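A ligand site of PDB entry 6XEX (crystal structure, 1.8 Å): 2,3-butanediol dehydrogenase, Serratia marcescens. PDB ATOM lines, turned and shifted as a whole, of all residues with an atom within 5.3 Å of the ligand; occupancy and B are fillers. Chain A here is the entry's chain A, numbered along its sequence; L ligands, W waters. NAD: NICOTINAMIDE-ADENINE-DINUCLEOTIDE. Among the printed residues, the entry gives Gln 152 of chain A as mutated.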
ATOM      1  N   GLY A  25     -22.587  20.303 -30.972  1.00  0.00           N
ATOM      2  CA  GLY A  25     -22.553  19.836 -29.571  1.00  0.00           C
ATOM      3  C   GLY A  25     -22.327  20.996 -28.621  1.00  0.00           C
ATOM      4  O   GLY A  25     -21.687  20.830 -27.568  1.00  0.00           O
ATOM      5  N   ALA A  26     -22.863  22.172 -28.961  1.00  0.00           N
ATOM      6  CA  ALA A  26     -22.549  23.407 -28.233  1.00  0.00           C
ATOM      7  C   ALA A  26     -23.427  23.526 -26.972  1.00  0.00           C
ATOM      8  O   ALA A  26     -23.205  24.495 -26.260  1.00  0.00           O
ATOM      9  CB  ALA A  26     -22.670  24.624 -29.126  1.00  0.00           C
ATOM     10  N   GLY A  27     -24.353  22.591 -26.714  1.00  0.00           N
ATOM     11  CA  GLY A  27     -25.306  22.682 -25.594  1.00  0.00           C
ATOM     12  C   GLY A  27     -24.679  22.266 -24.276  1.00  0.00           C
ATOM     13  O   GLY A  27     -25.224  22.614 -23.213  1.00  0.00           O
ATOM     14  N   ASN A  28     -23.509  21.632 -24.305  1.00  0.00           N
ATOM     15  CA  ASN A  28     -22.881  21.029 -23.094  1.00  0.00           C
ATOM     16  C   ASN A  28     -21.356  20.932 -23.261  1.00  0.00           C
ATOM     17  O   ASN A  28     -20.886  20.972 -24.412  1.00  0.00           O
ATOM     18  CB  ASN A  28     -23.426  19.624 -22.895  1.00  0.00           C
ATOM     19  CG  ASN A  28     -24.870  19.589 -22.447  1.00  0.00           C
ATOM     20  OD1 ASN A  28     -25.140  19.891 -21.283  1.00  0.00           O
ATOM     21  ND2 ASN A  28     -25.783  19.133 -23.302  1.00  0.00           N
ATOM     22  N   GLY A  29     -20.628  20.822 -22.154  1.00  0.00           N
ATOM     23  CA  GLY A  29     -19.235  20.305 -22.155  1.00  0.00           C
ATOM     24  C   GLY A  29     -18.263  21.160 -22.961  1.00  0.00           C
ATOM     25  O   GLY A  29     -18.282  22.416 -22.851  1.00  0.00           O
ATOM     26  N   MET A  30     -17.424  20.530 -23.797  1.00  0.00           N
ATOM     27  CA  MET A  30     -16.398  21.254 -24.572  1.00  0.00           C
ATOM     28  C   MET A  30     -17.031  22.157 -25.633  1.00  0.00           C
ATOM     29  O   MET A  30     -16.484  23.229 -25.841  1.00  0.00           O
ATOM     30  CB  MET A  30     -15.413  20.256 -25.190  1.00  0.00           C
ATOM     31  CG  MET A  30     -14.434  19.739 -24.151  1.00  0.00           C
ATOM     32  SD  MET A  30     -13.349  18.495 -24.857  1.00  0.00           S
ATOM     33  CE  MET A  30     -14.295  17.023 -24.498  1.00  0.00           C
ATOM     34  N   GLY A  31     -18.152  21.769 -26.263  1.00  0.00           N
ATOM     35  CA  GLY A  31     -18.806  22.666 -27.239  1.00  0.00           C
ATOM     36  C   GLY A  31     -19.312  23.940 -26.550  1.00  0.00           C
ATOM     37  O   GLY A  31     -19.167  25.019 -27.115  1.00  0.00           O
ATOM     38  N   ALA A  48     -25.171  24.532 -32.536  1.00  0.00           N
ATOM     39  CA  ALA A  48     -25.927  23.402 -33.096  1.00  0.00           C
ATOM     40  C   ALA A  48     -25.920  22.271 -32.071  1.00  0.00           C
ATOM     41  O   ALA A  48     -24.827  21.879 -31.612  1.00  0.00           O
ATOM     42  CB  ALA A  48     -25.360  22.960 -34.428  1.00  0.00           C
ATOM     43  N   ASP A  49     -27.098  21.775 -31.713  1.00  0.00           N
ATOM     44  CA  ASP A  49     -27.212  20.619 -30.785  1.00  0.00           C
ATOM     45  C   ASP A  49     -28.593  20.000 -30.910  1.00  0.00           C
ATOM     46  O   ASP A  49     -29.526  20.722 -31.368  1.00  0.00           O
ATOM     47  CB  ASP A  49     -26.977  21.030 -29.339  1.00  0.00           C
ATOM     48  CG  ASP A  49     -26.421  19.942 -28.455  1.00  0.00           C
ATOM     49  OD1 ASP A  49     -27.125  18.904 -28.234  1.00  0.00           O
ATOM     50  OD2 ASP A  49     -25.279  20.164 -27.929  1.00  0.00           O
ATOM     51  N   TRP A  50     -28.695  18.720 -30.568  1.00  0.00           N
ATOM     52  CA  TRP A  50     -29.984  17.991 -30.548  1.00  0.00           C
ATOM     53  C   TRP A  50     -30.612  18.069 -29.144  1.00  0.00           C
ATOM     54  O   TRP A  50     -31.792  17.691 -29.037  1.00  0.00           O
ATOM     55  CB  TRP A  50     -29.820  16.588 -31.130  1.00  0.00           C
ATOM     56  CG  TRP A  50     -29.048  15.547 -30.364  1.00  0.00           C
ATOM     57  CD1 TRP A  50     -28.304  15.669 -29.223  1.00  0.00           C
ATOM     58  CD2 TRP A  50     -28.908  14.187 -30.785  1.00  0.00           C
ATOM     59  NE1 TRP A  50     -27.744  14.467 -28.893  1.00  0.00           N
ATOM     60  CE2 TRP A  50     -28.094  13.523 -29.832  1.00  0.00           C
ATOM     61  CE3 TRP A  50     -29.420  13.448 -31.861  1.00  0.00           C
ATOM     62  CZ2 TRP A  50     -27.800  12.163 -29.928  1.00  0.00           C
ATOM     63  CZ3 TRP A  50     -29.140  12.097 -31.957  1.00  0.00           C
ATOM     64  CH2 TRP A  50     -28.338  11.469 -30.988  1.00  0.00           C
ATOM     65  N   ALA A  51     -29.901  18.600 -28.151  1.00  0.00           N
ATOM     66  CA  ALA A  51     -30.421  18.848 -26.788  1.00  0.00           C
ATOM     67  C   ALA A  51     -30.977  20.277 -26.760  1.00  0.00           C
ATOM     68  O   ALA A  51     -30.223  21.218 -26.476  1.00  0.00           O
ATOM     69  CB  ALA A  51     -29.356  18.641 -25.742  1.00  0.00           C
ATOM     70  N   ILE A  72     -30.626  20.553 -34.153  1.00  0.00           N
ATOM     71  CA  ILE A  72     -30.227  19.644 -35.280  1.00  0.00           C
ATOM     72  C   ILE A  72     -29.547  18.369 -34.742  1.00  0.00           C
ATOM     73  O   ILE A  72     -28.838  18.432 -33.727  1.00  0.00           O
ATOM     74  CB  ILE A  72     -29.314  20.375 -36.285  1.00  0.00           C
ATOM     75  CG1 ILE A  72     -28.953  19.510 -37.499  1.00  0.00           C
ATOM     76  CG2 ILE A  72     -28.074  20.964 -35.624  1.00  0.00           C
ATOM     77  CD1 ILE A  72     -28.307  20.310 -38.642  1.00  0.00           C
ATOM     78  N   ASP A  73     -29.798  17.267 -35.442  1.00  0.00           N
ATOM     79  CA  ASP A  73     -29.078  15.972 -35.373  1.00  0.00           C
ATOM     80  C   ASP A  73     -28.040  15.995 -36.498  1.00  0.00           C
ATOM     81  O   ASP A  73     -28.415  15.851 -37.690  1.00  0.00           O
ATOM     82  CB  ASP A  73     -30.046  14.804 -35.499  1.00  0.00           C
ATOM     83  CG  ASP A  73     -29.374  13.443 -35.440  1.00  0.00           C
ATOM     84  OD1 ASP A  73     -28.120  13.397 -35.478  1.00  0.00           O
ATOM     85  OD2 ASP A  73     -30.088  12.448 -35.397  1.00  0.00           O
ATOM     86  N   VAL A  74     -26.765  16.184 -36.164  1.00  0.00           N
ATOM     87  CA  VAL A  74     -25.730  16.368 -37.198  1.00  0.00           C
ATOM     88  C   VAL A  74     -25.517  15.067 -37.995  1.00  0.00           C
ATOM     89  O   VAL A  74     -24.814  15.157 -39.030  1.00  0.00           O
ATOM     90  CB  VAL A  74     -24.406  16.863 -36.579  1.00  0.00           C
ATOM     91  CG1 VAL A  74     -24.568  18.247 -36.003  1.00  0.00           C
ATOM     92  CG2 VAL A  74     -23.879  15.886 -35.551  1.00  0.00           C
ATOM     93  N   SER A  75     -26.097  13.941 -37.583  1.00  0.00           N
ATOM     94  CA  SER A  75     -26.022  12.672 -38.355  1.00  0.00           C
ATOM     95  C   SER A  75     -26.857  12.767 -39.651  1.00  0.00           C
ATOM     96  O   SER A  75     -26.711  11.889 -40.545  1.00  0.00           O
ATOM     97  CB  SER A  75     -26.421  11.449 -37.537  1.00  0.00           C
ATOM     98  OG  SER A  75     -27.829  11.333 -37.291  1.00  0.00           O
ATOM     99  N   ASN A 100     -17.733  19.078 -33.065  1.00  0.00           N
ATOM    100  CA  ASN A 100     -17.508  18.711 -31.656  1.00  0.00           C
ATOM    101  C   ASN A 100     -18.540  17.693 -31.191  1.00  0.00           C
ATOM    102  O   ASN A 100     -18.233  16.947 -30.268  1.00  0.00           O
ATOM    103  CB  ASN A 100     -17.438  19.975 -30.822  1.00  0.00           C
ATOM    104  CG  ASN A 100     -17.422  19.647 -29.364  1.00  0.00           C
ATOM    105  OD1 ASN A 100     -16.386  19.242 -28.847  1.00  0.00           O
ATOM    106  ND2 ASN A 100     -18.588  19.791 -28.725  1.00  0.00           N
ATOM    107  N   ALA A 101     -19.750  17.676 -31.758  1.00  0.00           N
ATOM    108  CA  ALA A 101     -20.847  16.802 -31.338  1.00  0.00           C
ATOM    109  C   ALA A 101     -20.342  15.346 -31.363  1.00  0.00           C
ATOM    110  O   ALA A 101     -19.668  14.969 -32.321  1.00  0.00           O
ATOM    111  CB  ALA A 101     -22.068  16.971 -32.242  1.00  0.00           C
ATOM    112  N   GLY A 102     -20.709  14.583 -30.357  1.00  0.00           N
ATOM    113  CA  GLY A 102     -20.206  13.216 -30.224  1.00  0.00           C
ATOM    114  C   GLY A 102     -21.008  12.491 -29.169  1.00  0.00           C
ATOM    115  O   GLY A 102     -21.568  13.177 -28.258  1.00  0.00           O
ATOM    116  N   VAL A 103     -21.066  11.176 -29.316  1.00  0.00           N
ATOM    117  CA  VAL A 103     -21.620  10.245 -28.301  1.00  0.00           C
ATOM    118  C   VAL A 103     -20.616   9.140 -28.043  1.00  0.00           C
ATOM    119  O   VAL A 103     -19.736   8.890 -28.874  1.00  0.00           O
ATOM    120  CB  VAL A 103     -22.961   9.642 -28.778  1.00  0.00           C
ATOM    121  CG1 VAL A 103     -24.050  10.683 -28.886  1.00  0.00           C
ATOM    122  CG2 VAL A 103     -22.834   8.923 -30.096  1.00  0.00           C
ATOM    123  N   VAL A 123     -23.270   9.834 -35.588  1.00  0.00           N
ATOM    124  CA  VAL A 123     -22.892  11.135 -34.983  1.00  0.00           C
ATOM    125  C   VAL A 123     -21.390  11.403 -35.182  1.00  0.00           C
ATOM    126  O   VAL A 123     -21.059  12.442 -35.694  1.00  0.00           O
ATOM    127  CB  VAL A 123     -23.255  11.170 -33.494  1.00  0.00           C
ATOM    128  CG1 VAL A 123     -22.855  12.516 -32.892  1.00  0.00           C
ATOM    129  CG2 VAL A 123     -24.732  10.869 -33.248  1.00  0.00           C
ATOM    130  N   ASP A 124     -20.545  10.474 -34.728  1.00  0.00           N
ATOM    131  CA  ASP A 124     -19.087  10.685 -34.581  1.00  0.00           C
ATOM    132  C   ASP A 124     -18.378  10.665 -35.940  1.00  0.00           C
ATOM    133  O   ASP A 124     -17.372  11.372 -36.048  1.00  0.00           O
ATOM    134  CB  ASP A 124     -18.474   9.692 -33.577  1.00  0.00           C
ATOM    135  CG  ASP A 124     -19.077   9.711 -32.179  1.00  0.00           C
ATOM    136  OD1 ASP A 124     -19.879  10.583 -31.918  1.00  0.00           O
ATOM    137  OD2 ASP A 124     -18.713   8.802 -31.357  1.00  0.00           O
ATOM    138  N   THR A 149     -13.267  17.767 -33.037  1.00  0.00           N
ATOM    139  CA  THR A 149     -13.013  17.083 -31.747  1.00  0.00           C
ATOM    140  C   THR A 149     -12.830  15.601 -32.031  1.00  0.00           C
ATOM    141  O   THR A 149     -13.835  14.875 -32.135  1.00  0.00           O
ATOM    142  CB  THR A 149     -14.070  17.353 -30.661  1.00  0.00           C
ATOM    143  OG1 THR A 149     -14.226  18.768 -30.668  1.00  0.00           O
ATOM    144  CG2 THR A 149     -13.581  16.860 -29.308  1.00  0.00           C
ATOM    145  N   ALA A 150     -11.599  15.138 -32.120  1.00  0.00           N
ATOM    146  CA  ALA A 150     -11.336  13.684 -32.193  1.00  0.00           C
ATOM    147  C   ALA A 150     -11.213  13.220 -30.739  1.00  0.00           C
ATOM    148  O   ALA A 150     -12.109  13.564 -29.912  1.00  0.00           O
ATOM    149  CB  ALA A 150     -10.109  13.412 -33.012  1.00  0.00           C
ATOM    150  N   SER A 151     -10.145  12.536 -30.397  1.00  0.00           N
ATOM    151  CA  SER A 151      -9.962  11.947 -29.063  1.00  0.00           C
ATOM    152  C   SER A 151      -8.599  11.293 -29.039  1.00  0.00           C
ATOM    153  O   SER A 151      -8.130  10.837 -30.078  1.00  0.00           O
ATOM    154  CB  SER A 151     -10.978  10.915 -28.721  1.00  0.00           C
ATOM    155  OG  SER A 151     -10.734  10.355 -27.431  1.00  0.00           O
ATOM    156  N   GLN A 152      -8.046  11.148 -27.839  1.00  0.00           N
ATOM    157  CA  GLN A 152      -6.988  10.136 -27.630  1.00  0.00           C
ATOM    158  C   GLN A 152      -7.428   8.813 -28.249  1.00  0.00           C
ATOM    159  O   GLN A 152      -6.586   8.153 -28.849  1.00  0.00           O
ATOM    160  CB  GLN A 152      -6.650  10.040 -26.144  1.00  0.00           C
ATOM    161  CG  GLN A 152      -7.068   8.792 -25.453  1.00  0.00           C
ATOM    162  CD  GLN A 152      -6.725   8.789 -23.996  1.00  0.00           C
ATOM    163  OE1 GLN A 152      -7.547   9.152 -23.175  1.00  0.00           O
ATOM    164  NE2 GLN A 152      -5.537   8.317 -23.656  1.00  0.00           N
ATOM    165  N   TYR A 164     -16.395   3.337 -30.784  1.00  0.00           N
ATOM    166  CA  TYR A 164     -15.905   4.726 -30.536  1.00  0.00           C
ATOM    167  C   TYR A 164     -14.499   4.901 -31.145  1.00  0.00           C
ATOM    168  O   TYR A 164     -14.214   5.929 -31.740  1.00  0.00           O
ATOM    169  CB  TYR A 164     -15.900   5.022 -29.029  1.00  0.00           C
ATOM    170  CG  TYR A 164     -15.526   6.437 -28.662  1.00  0.00           C
ATOM    171  CD1 TYR A 164     -16.421   7.467 -28.912  1.00  0.00           C
ATOM    172  CD2 TYR A 164     -14.347   6.736 -27.995  1.00  0.00           C
ATOM    173  CE1 TYR A 164     -16.122   8.774 -28.559  1.00  0.00           C
ATOM    174  CE2 TYR A 164     -14.040   8.044 -27.610  1.00  0.00           C
ATOM    175  CZ  TYR A 164     -14.935   9.062 -27.925  1.00  0.00           C
ATOM    176  OH  TYR A 164     -14.717  10.347 -27.560  1.00  0.00           O
ATOM    177  N   LYS A 168     -13.471   7.601 -33.954  1.00  0.00           N
ATOM    178  CA  LYS A 168     -12.497   8.673 -33.721  1.00  0.00           C
ATOM    179  C   LYS A 168     -11.276   8.434 -34.615  1.00  0.00           C
ATOM    180  O   LYS A 168     -10.636   9.446 -35.080  1.00  0.00           O
ATOM    181  CB  LYS A 168     -12.186   8.773 -32.230  1.00  0.00           C
ATOM    182  CG  LYS A 168     -13.337   9.255 -31.386  1.00  0.00           C
ATOM    183  CD  LYS A 168     -13.801  10.660 -31.802  1.00  0.00           C
ATOM    184  CE  LYS A 168     -14.765  11.261 -30.806  1.00  0.00           C
ATOM    185  NZ  LYS A 168     -15.218  12.585 -31.262  1.00  0.00           N
ATOM    186  N   PRO A 194      -8.433  15.098 -26.969  1.00  0.00           N
ATOM    187  CA  PRO A 194      -8.364  15.049 -25.515  1.00  0.00           C
ATOM    188  C   PRO A 194      -8.286  13.630 -24.971  1.00  0.00           C
ATOM    189  O   PRO A 194      -8.759  12.655 -25.605  1.00  0.00           O
ATOM    190  CB  PRO A 194      -9.646  15.764 -25.028  1.00  0.00           C
ATOM    191  CG  PRO A 194     -10.167  16.435 -26.291  1.00  0.00           C
ATOM    192  CD  PRO A 194      -9.758  15.543 -27.434  1.00  0.00           C
ATOM    193  N   SER A 195      -7.742  13.535 -23.765  1.00  0.00           N
ATOM    194  CA  SER A 195      -7.927  12.362 -22.905  1.00  0.00           C
ATOM    195  C   SER A 195      -9.171  12.704 -22.081  1.00  0.00           C
ATOM    196  O   SER A 195     -10.067  13.405 -22.630  1.00  0.00           O
ATOM    197  CB  SER A 195      -6.704  12.053 -22.023  1.00  0.00           C
ATOM    198  OG  SER A 195      -6.913  10.811 -21.359  1.00  0.00           O
ATOM    199  N   LEU A 196      -9.227  12.240 -20.853  1.00  0.00           N
ATOM    200  CA  LEU A 196     -10.428  12.423 -20.010  1.00  0.00           C
ATOM    201  C   LEU A 196     -10.677  13.904 -19.781  1.00  0.00           C
ATOM    202  O   LEU A 196      -9.761  14.609 -19.392  1.00  0.00           O
ATOM    203  CB  LEU A 196     -10.240  11.678 -18.680  1.00  0.00           C
ATOM    204  CG  LEU A 196     -11.422  11.734 -17.723  1.00  0.00           C
ATOM    205  CD1 LEU A 196     -12.668  11.146 -18.356  1.00  0.00           C
ATOM    206  CD2 LEU A 196     -11.114  10.972 -16.439  1.00  0.00           C
ATOM    207  N   VAL A 197     -11.926  14.329 -19.983  1.00  0.00           N
ATOM    208  CA  VAL A 197     -12.409  15.689 -19.740  1.00  0.00           C
ATOM    209  C   VAL A 197     -13.623  15.615 -18.817  1.00  0.00           C
ATOM    210  O   VAL A 197     -14.429  14.704 -18.974  1.00  0.00           O
ATOM    211  CB  VAL A 197     -12.766  16.392 -21.055  1.00  0.00           C
ATOM    212  CG1 VAL A 197     -13.067  17.866 -20.854  1.00  0.00           C
ATOM    213  CG2 VAL A 197     -11.616  16.197 -22.049  1.00  0.00           C
ATOM    214  N   LYS A 198     -13.760  16.595 -17.942  1.00  0.00           N
ATOM    215  CA  LYS A 198     -14.909  16.637 -16.997  1.00  0.00           C
ATOM    216  C   LYS A 198     -16.199  17.108 -17.673  1.00  0.00           C
ATOM    217  O   LYS A 198     -16.471  18.317 -17.629  1.00  0.00           O
ATOM    218  CB  LYS A 198     -14.526  17.596 -15.893  1.00  0.00           C
ATOM    219  CG  LYS A 198     -13.466  17.041 -14.978  1.00  0.00           C
ATOM    220  CD  LYS A 198     -13.140  18.101 -13.946  1.00  0.00           C
ATOM    221  CE  LYS A 198     -11.866  17.805 -13.193  1.00  0.00           C
ATOM    222  NZ  LYS A 198     -11.675  18.815 -12.110  1.00  0.00           N
ATOM    223  N   THR A 199     -16.935  16.193 -18.280  1.00  0.00           N
ATOM    224  CA  THR A 199     -18.165  16.482 -19.063  1.00  0.00           C
ATOM    225  C   THR A 199     -19.207  15.408 -18.764  1.00  0.00           C
ATOM    226  O   THR A 199     -18.839  14.357 -18.162  1.00  0.00           O
ATOM    227  CB  THR A 199     -17.907  16.550 -20.581  1.00  0.00           C
ATOM    228  OG1 THR A 199     -17.782  15.228 -21.129  1.00  0.00           O
ATOM    229  CG2 THR A 199     -16.694  17.350 -20.961  1.00  0.00           C
ATOM    230  N   ASN A 200     -20.441  15.651 -19.227  1.00  0.00           N
ATOM    231  CA  ASN A 200     -21.542  14.676 -19.268  1.00  0.00           C
ATOM    232  C   ASN A 200     -21.101  13.344 -19.892  1.00  0.00           C
ATOM    233  O   ASN A 200     -21.556  12.299 -19.433  1.00  0.00           O
ATOM    234  CB  ASN A 200     -22.766  15.195 -20.012  1.00  0.00           C
ATOM    235  CG  ASN A 200     -23.489  16.268 -19.218  1.00  0.00           C
ATOM    236  OD1 ASN A 200     -23.226  16.475 -18.023  1.00  0.00           O
ATOM    237  ND2 ASN A 200     -24.374  16.984 -19.880  1.00  0.00           N
ATOM    238  N   MET A 201     -20.177  13.344 -20.837  1.00  0.00           N
ATOM    239  CA  MET A 201     -19.792  12.094 -21.538  1.00  0.00           C
ATOM    240  C   MET A 201     -19.208  11.064 -20.560  1.00  0.00           C
ATOM    241  O   MET A 201     -19.409   9.843 -20.786  1.00  0.00           O
ATOM    242  CB  MET A 201     -18.825  12.393 -22.695  1.00  0.00           C
ATOM    243  CG  MET A 201     -18.589  11.151 -23.505  1.00  0.00           C
ATOM    244  SD  MET A 201     -17.769  11.363 -25.074  1.00  0.00           S
ATOM    245  CE  MET A 201     -19.151  11.968 -26.048  1.00  0.00           C
ATOM    246  N   THR A 202     -18.509  11.503 -19.509  1.00  0.00           N
ATOM    247  CA  THR A 202     -17.693  10.667 -18.612  1.00  0.00           C
ATOM    248  C   THR A 202     -18.170  10.767 -17.166  1.00  0.00           C
ATOM    249  O   THR A 202     -17.604  10.095 -16.334  1.00  0.00           O
ATOM    250  CB  THR A 202     -16.229  11.104 -18.756  1.00  0.00           C
ATOM    251  OG1 THR A 202     -16.224  12.504 -18.456  1.00  0.00           O
ATOM    252  CG2 THR A 202     -15.680  10.858 -20.150  1.00  0.00           C
HETATM  253  PA  NAD L   1     -21.072  16.413 -23.640  1.00  0.00           P
HETATM  254  O1A NAD L   1     -22.006  15.269 -23.453  1.00  0.00           O
HETATM  255  O2A NAD L   1     -20.846  17.394 -22.551  1.00  0.00           O
HETATM  256  O5B NAD L   1     -21.362  17.291 -24.920  1.00  0.00           O
HETATM  257  C5B NAD L   1     -21.602  16.696 -26.176  1.00  0.00           C
HETATM  258  C4B NAD L   1     -22.714  17.472 -26.833  1.00  0.00           C
HETATM  259  O4B NAD L   1     -22.927  16.981 -28.178  1.00  0.00           O
HETATM  260  C3B NAD L   1     -24.064  17.360 -26.099  1.00  0.00           C
HETATM  261  O3B NAD L   1     -24.596  18.661 -25.887  1.00  0.00           O
HETATM  262  C2B NAD L   1     -24.928  16.541 -27.062  1.00  0.00           C
HETATM  263  O2B NAD L   1     -26.297  16.822 -26.866  1.00  0.00           O
HETATM  264  C1B NAD L   1     -24.316  16.930 -28.416  1.00  0.00           C
HETATM  265  N9A NAD L   1     -24.623  15.963 -29.474  1.00  0.00           N
HETATM  266  C8A NAD L   1     -24.480  14.619 -29.394  1.00  0.00           C
HETATM  267  N7A NAD L   1     -24.903  13.979 -30.455  1.00  0.00           N
HETATM  268  C5A NAD L   1     -25.390  14.973 -31.285  1.00  0.00           C
HETATM  269  C6A NAD L   1     -26.019  14.919 -32.545  1.00  0.00           C
HETATM  270  N6A NAD L   1     -26.323  13.799 -33.203  1.00  0.00           N
HETATM  271  N1A NAD L   1     -26.402  16.103 -33.068  1.00  0.00           N
HETATM  272  C2A NAD L   1     -26.156  17.230 -32.383  1.00  0.00           C
HETATM  273  N3A NAD L   1     -25.599  17.393 -31.196  1.00  0.00           N
HETATM  274  C4A NAD L   1     -25.230  16.209 -30.676  1.00  0.00           C
HETATM  275  O3  NAD L   1     -19.676  15.660 -23.931  1.00  0.00           O
HETATM  276  PN  NAD L   1     -18.275  16.256 -24.410  1.00  0.00           P
HETATM  277  O1N NAD L   1     -18.164  17.753 -24.290  1.00  0.00           O
HETATM  278  O2N NAD L   1     -17.336  15.416 -23.631  1.00  0.00           O
HETATM  279  O5D NAD L   1     -18.207  15.781 -25.960  1.00  0.00           O
HETATM  280  C5D NAD L   1     -17.766  16.616 -27.009  1.00  0.00           C
HETATM  281  C4D NAD L   1     -16.777  15.876 -27.884  1.00  0.00           C
HETATM  282  O4D NAD L   1     -15.576  15.573 -27.097  1.00  0.00           O
HETATM  283  C3D NAD L   1     -17.267  14.539 -28.473  1.00  0.00           C
HETATM  284  O3D NAD L   1     -16.976  14.414 -29.864  1.00  0.00           O
HETATM  285  C2D NAD L   1     -16.488  13.521 -27.644  1.00  0.00           C
HETATM  286  O2D NAD L   1     -16.333  12.294 -28.323  1.00  0.00           O
HETATM  287  C1D NAD L   1     -15.186  14.279 -27.446  1.00  0.00           C
HETATM  288  N1N NAD L   1     -14.317  13.706 -26.398  1.00  0.00           N
HETATM  289  C2N NAD L   1     -14.741  13.571 -25.092  1.00  0.00           C
HETATM  290  C3N NAD L   1     -13.828  13.273 -24.104  1.00  0.00           C
HETATM  291  C7N NAD L   1     -14.200  13.326 -22.641  1.00  0.00           C
HETATM  292  O7N NAD L   1     -13.508  12.678 -21.848  1.00  0.00           O
HETATM  293  N7N NAD L   1     -15.281  14.018 -22.290  1.00  0.00           N
HETATM  294  C4N NAD L   1     -12.531  12.903 -24.444  1.00  0.00           C
HETATM  295  C5N NAD L   1     -12.119  13.019 -25.758  1.00  0.00           C
HETATM  296  C6N NAD L   1     -13.005  13.448 -26.721  1.00  0.00           C
HETATM  297  O   HOH W   1     -26.821  15.939 -24.519  1.00  0.00           O
HETATM  298  O   HOH W   2     -20.959  18.348 -20.002  1.00  0.00           O
HETATM  299  O   HOH W   3     -17.098  15.200 -33.093  1.00  0.00           O
HETATM  300  O   HOH W   4     -24.625  15.830 -22.678  1.00  0.00           O
HETATM  301  O   HOH W   5     -22.500  12.655 -23.715  1.00  0.00           O
HETATM  302  O   HOH W   6     -19.516  19.227 -26.207  1.00  0.00           O
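Water W2 lies within hydrogen-bond range of O2A of the ligand (2.7 Å), N of Asn 200 (2.9 Å) and N of Gly 29 (3.3 Å).
Water W4 lies within hydrogen-bond range of O1A of the ligand (2.8 Å) and ND2 of Asn 200 (3.0 Å).
Water W3 lies within hydrogen-bond range of O of Ala 101 (2.7 Å), O3D of the ligand (3.3 Å) and O of Thr 149 (3.4 Å).
O of Ile 72 lies close to N1A of the ligand, at 3.4 Å.
CA of Gly 25 touches O4B of the ligand (3.2 Å).
C of Gly 27 touches O3B of the ligand, 3.9 Å away.
CB of Ala 51 touches O2B of the ligand, 3.7 Å away.
Ala 101 touches the ligand.
Gly 102 touches the ligand (O to C8A, 3.4 Å).
Val 103 touches the ligand.
CG2 of Val 123 touches N6A of the ligand (3.3 Å).
Thr 149 touches the ligand (CG2 to O4D, 3.2 Å).
O of Ala 150 touches C6N of the ligand, 3.3 Å away.
Ser 151 touches the ligand.
O of Pro 194 touches C5N of the ligand, at 3.4 Å.
O of Ser 195 touches C4N of the ligand, 3.1 Å away.
Leu 196 touches the ligand (CA to O7N, 3.6 Å).
Asn 200 touches the ligand (CB to O1A, 3.5 Å).
CG2 of Thr 202 touches O7N of the ligand, at 3.3 Å.
Hydrophobic or aromatic side chains within 4 Å of the ligand: Met 30, Trp 50, Ala 51, Val 74, Ala 101, Val 103, Val 123, Tyr 164, Pro 194, Leu 196, Val 197 and Met 201.
29 residues have an atom within 4 Å of the ligand: Gly 25, Gly 27, Asn 28, Gly 29, Met 30, Asp 49, Trp 50, Ala 51, Ile 72, Asp 73, Val 74, Asn 100, Ala 101, Gly 102, Val 103, Val 123, Thr 149, Ala 150, Ser 151, Tyr 164, Lys 168, Pro 194, Ser 195, Leu 196, Val 197, Thr 199, Asn 200, Met 201 and Thr 202.
The nearest printed residue that does not touch the ligand is Ser 75 (4.4 Å).
The backbone NH (N) of Met 201 is in hydrogen-bond range of the side-chain hydroxyl (OG1) of Thr 199.
The side-chain hydroxyl of Thr 149 is in hydrogen-bond range of the side-chain amide oxygen of Asn 100, 2.9 Å away.
OD1 of Asn 28 lies within hydrogen-bond range of ND2 of Asn 200, 3.3 Å away.
O of Val 197 sits at hydrogen-bond distance from OG1 of Thr 202.
O of Ala 48 lies within hydrogen-bond range of N of Gly 25 (2.8 Å).
O of Ile 72 sits at hydrogen-bond distance from N of Trp 50 (3.2 Å).
The backbone carbonyl oxygen (O) of Pro 194 lies within hydrogen-bond range of the backbone NH (N) of Gln 152, 2.8 Å away.
The backbone NH (N) of Val 103 sits at hydrogen-bond distance from the side-chain carboxylate (OD1) of Asp 124 (2.9 Å).
The side-chain hydroxyl (OG1) of Thr 199 is in hydrogen-bond range of an oxygen (O2N) of the ligand (2.5 Å).
The side-chain carboxylate of Asp 49 sits at hydrogen-bond distance from an oxygen (O2B) of the ligand.
The side-chain hydroxyl (OH) of Tyr 164 lies within hydrogen-bond range of an oxygen (O2D) of the ligand.
The backbone carbonyl oxygen of Asn 100 is in hydrogen-bond range of an oxygen (O3D) of the ligand (2.9 Å).
ND2 of Asn 28 is in hydrogen-bond range of O3B of the ligand (2.9 Å).
The side-chain amino group (NZ) of Lys 168 lies within hydrogen-bond range of an oxygen (O3D) of the ligand, 2.9 Å away.
N of Met 30 is in hydrogen-bond range of O1N of the ligand (2.9 Å).
OD1 of Asp 73 lies within hydrogen-bond range of N6A of the ligand.
An oxygen (O7N) of the ligand is in hydrogen-bond range of the backbone NH (N) of Val 197, 3.0 Å away.
The backbone carbonyl oxygen (O) of Val 197 sits at hydrogen-bond distance from a nitrogen (N7N) of the ligand, at 3.5 Å.
The backbone NH (N) of Val 74 sits at hydrogen-bond distance from a nitrogen (N1A) of the ligand (3.1 Å).
A nitrogen (N3A) of the ligand is in hydrogen-bond range of the backbone NH of Trp 50 (3.4 Å).
A nitrogen (N7A) of the ligand is in hydrogen-bond range of the indole nitrogen (NE1) of Trp 50 (3.3 Å).
An oxygen (O2A) of the ligand sits close to the backbone NH of Gly 29, at 3.5 Å.
An oxygen (O2D) of the ligand sits close to the side-chain sulfur of Met 201, 3.7 Å away.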
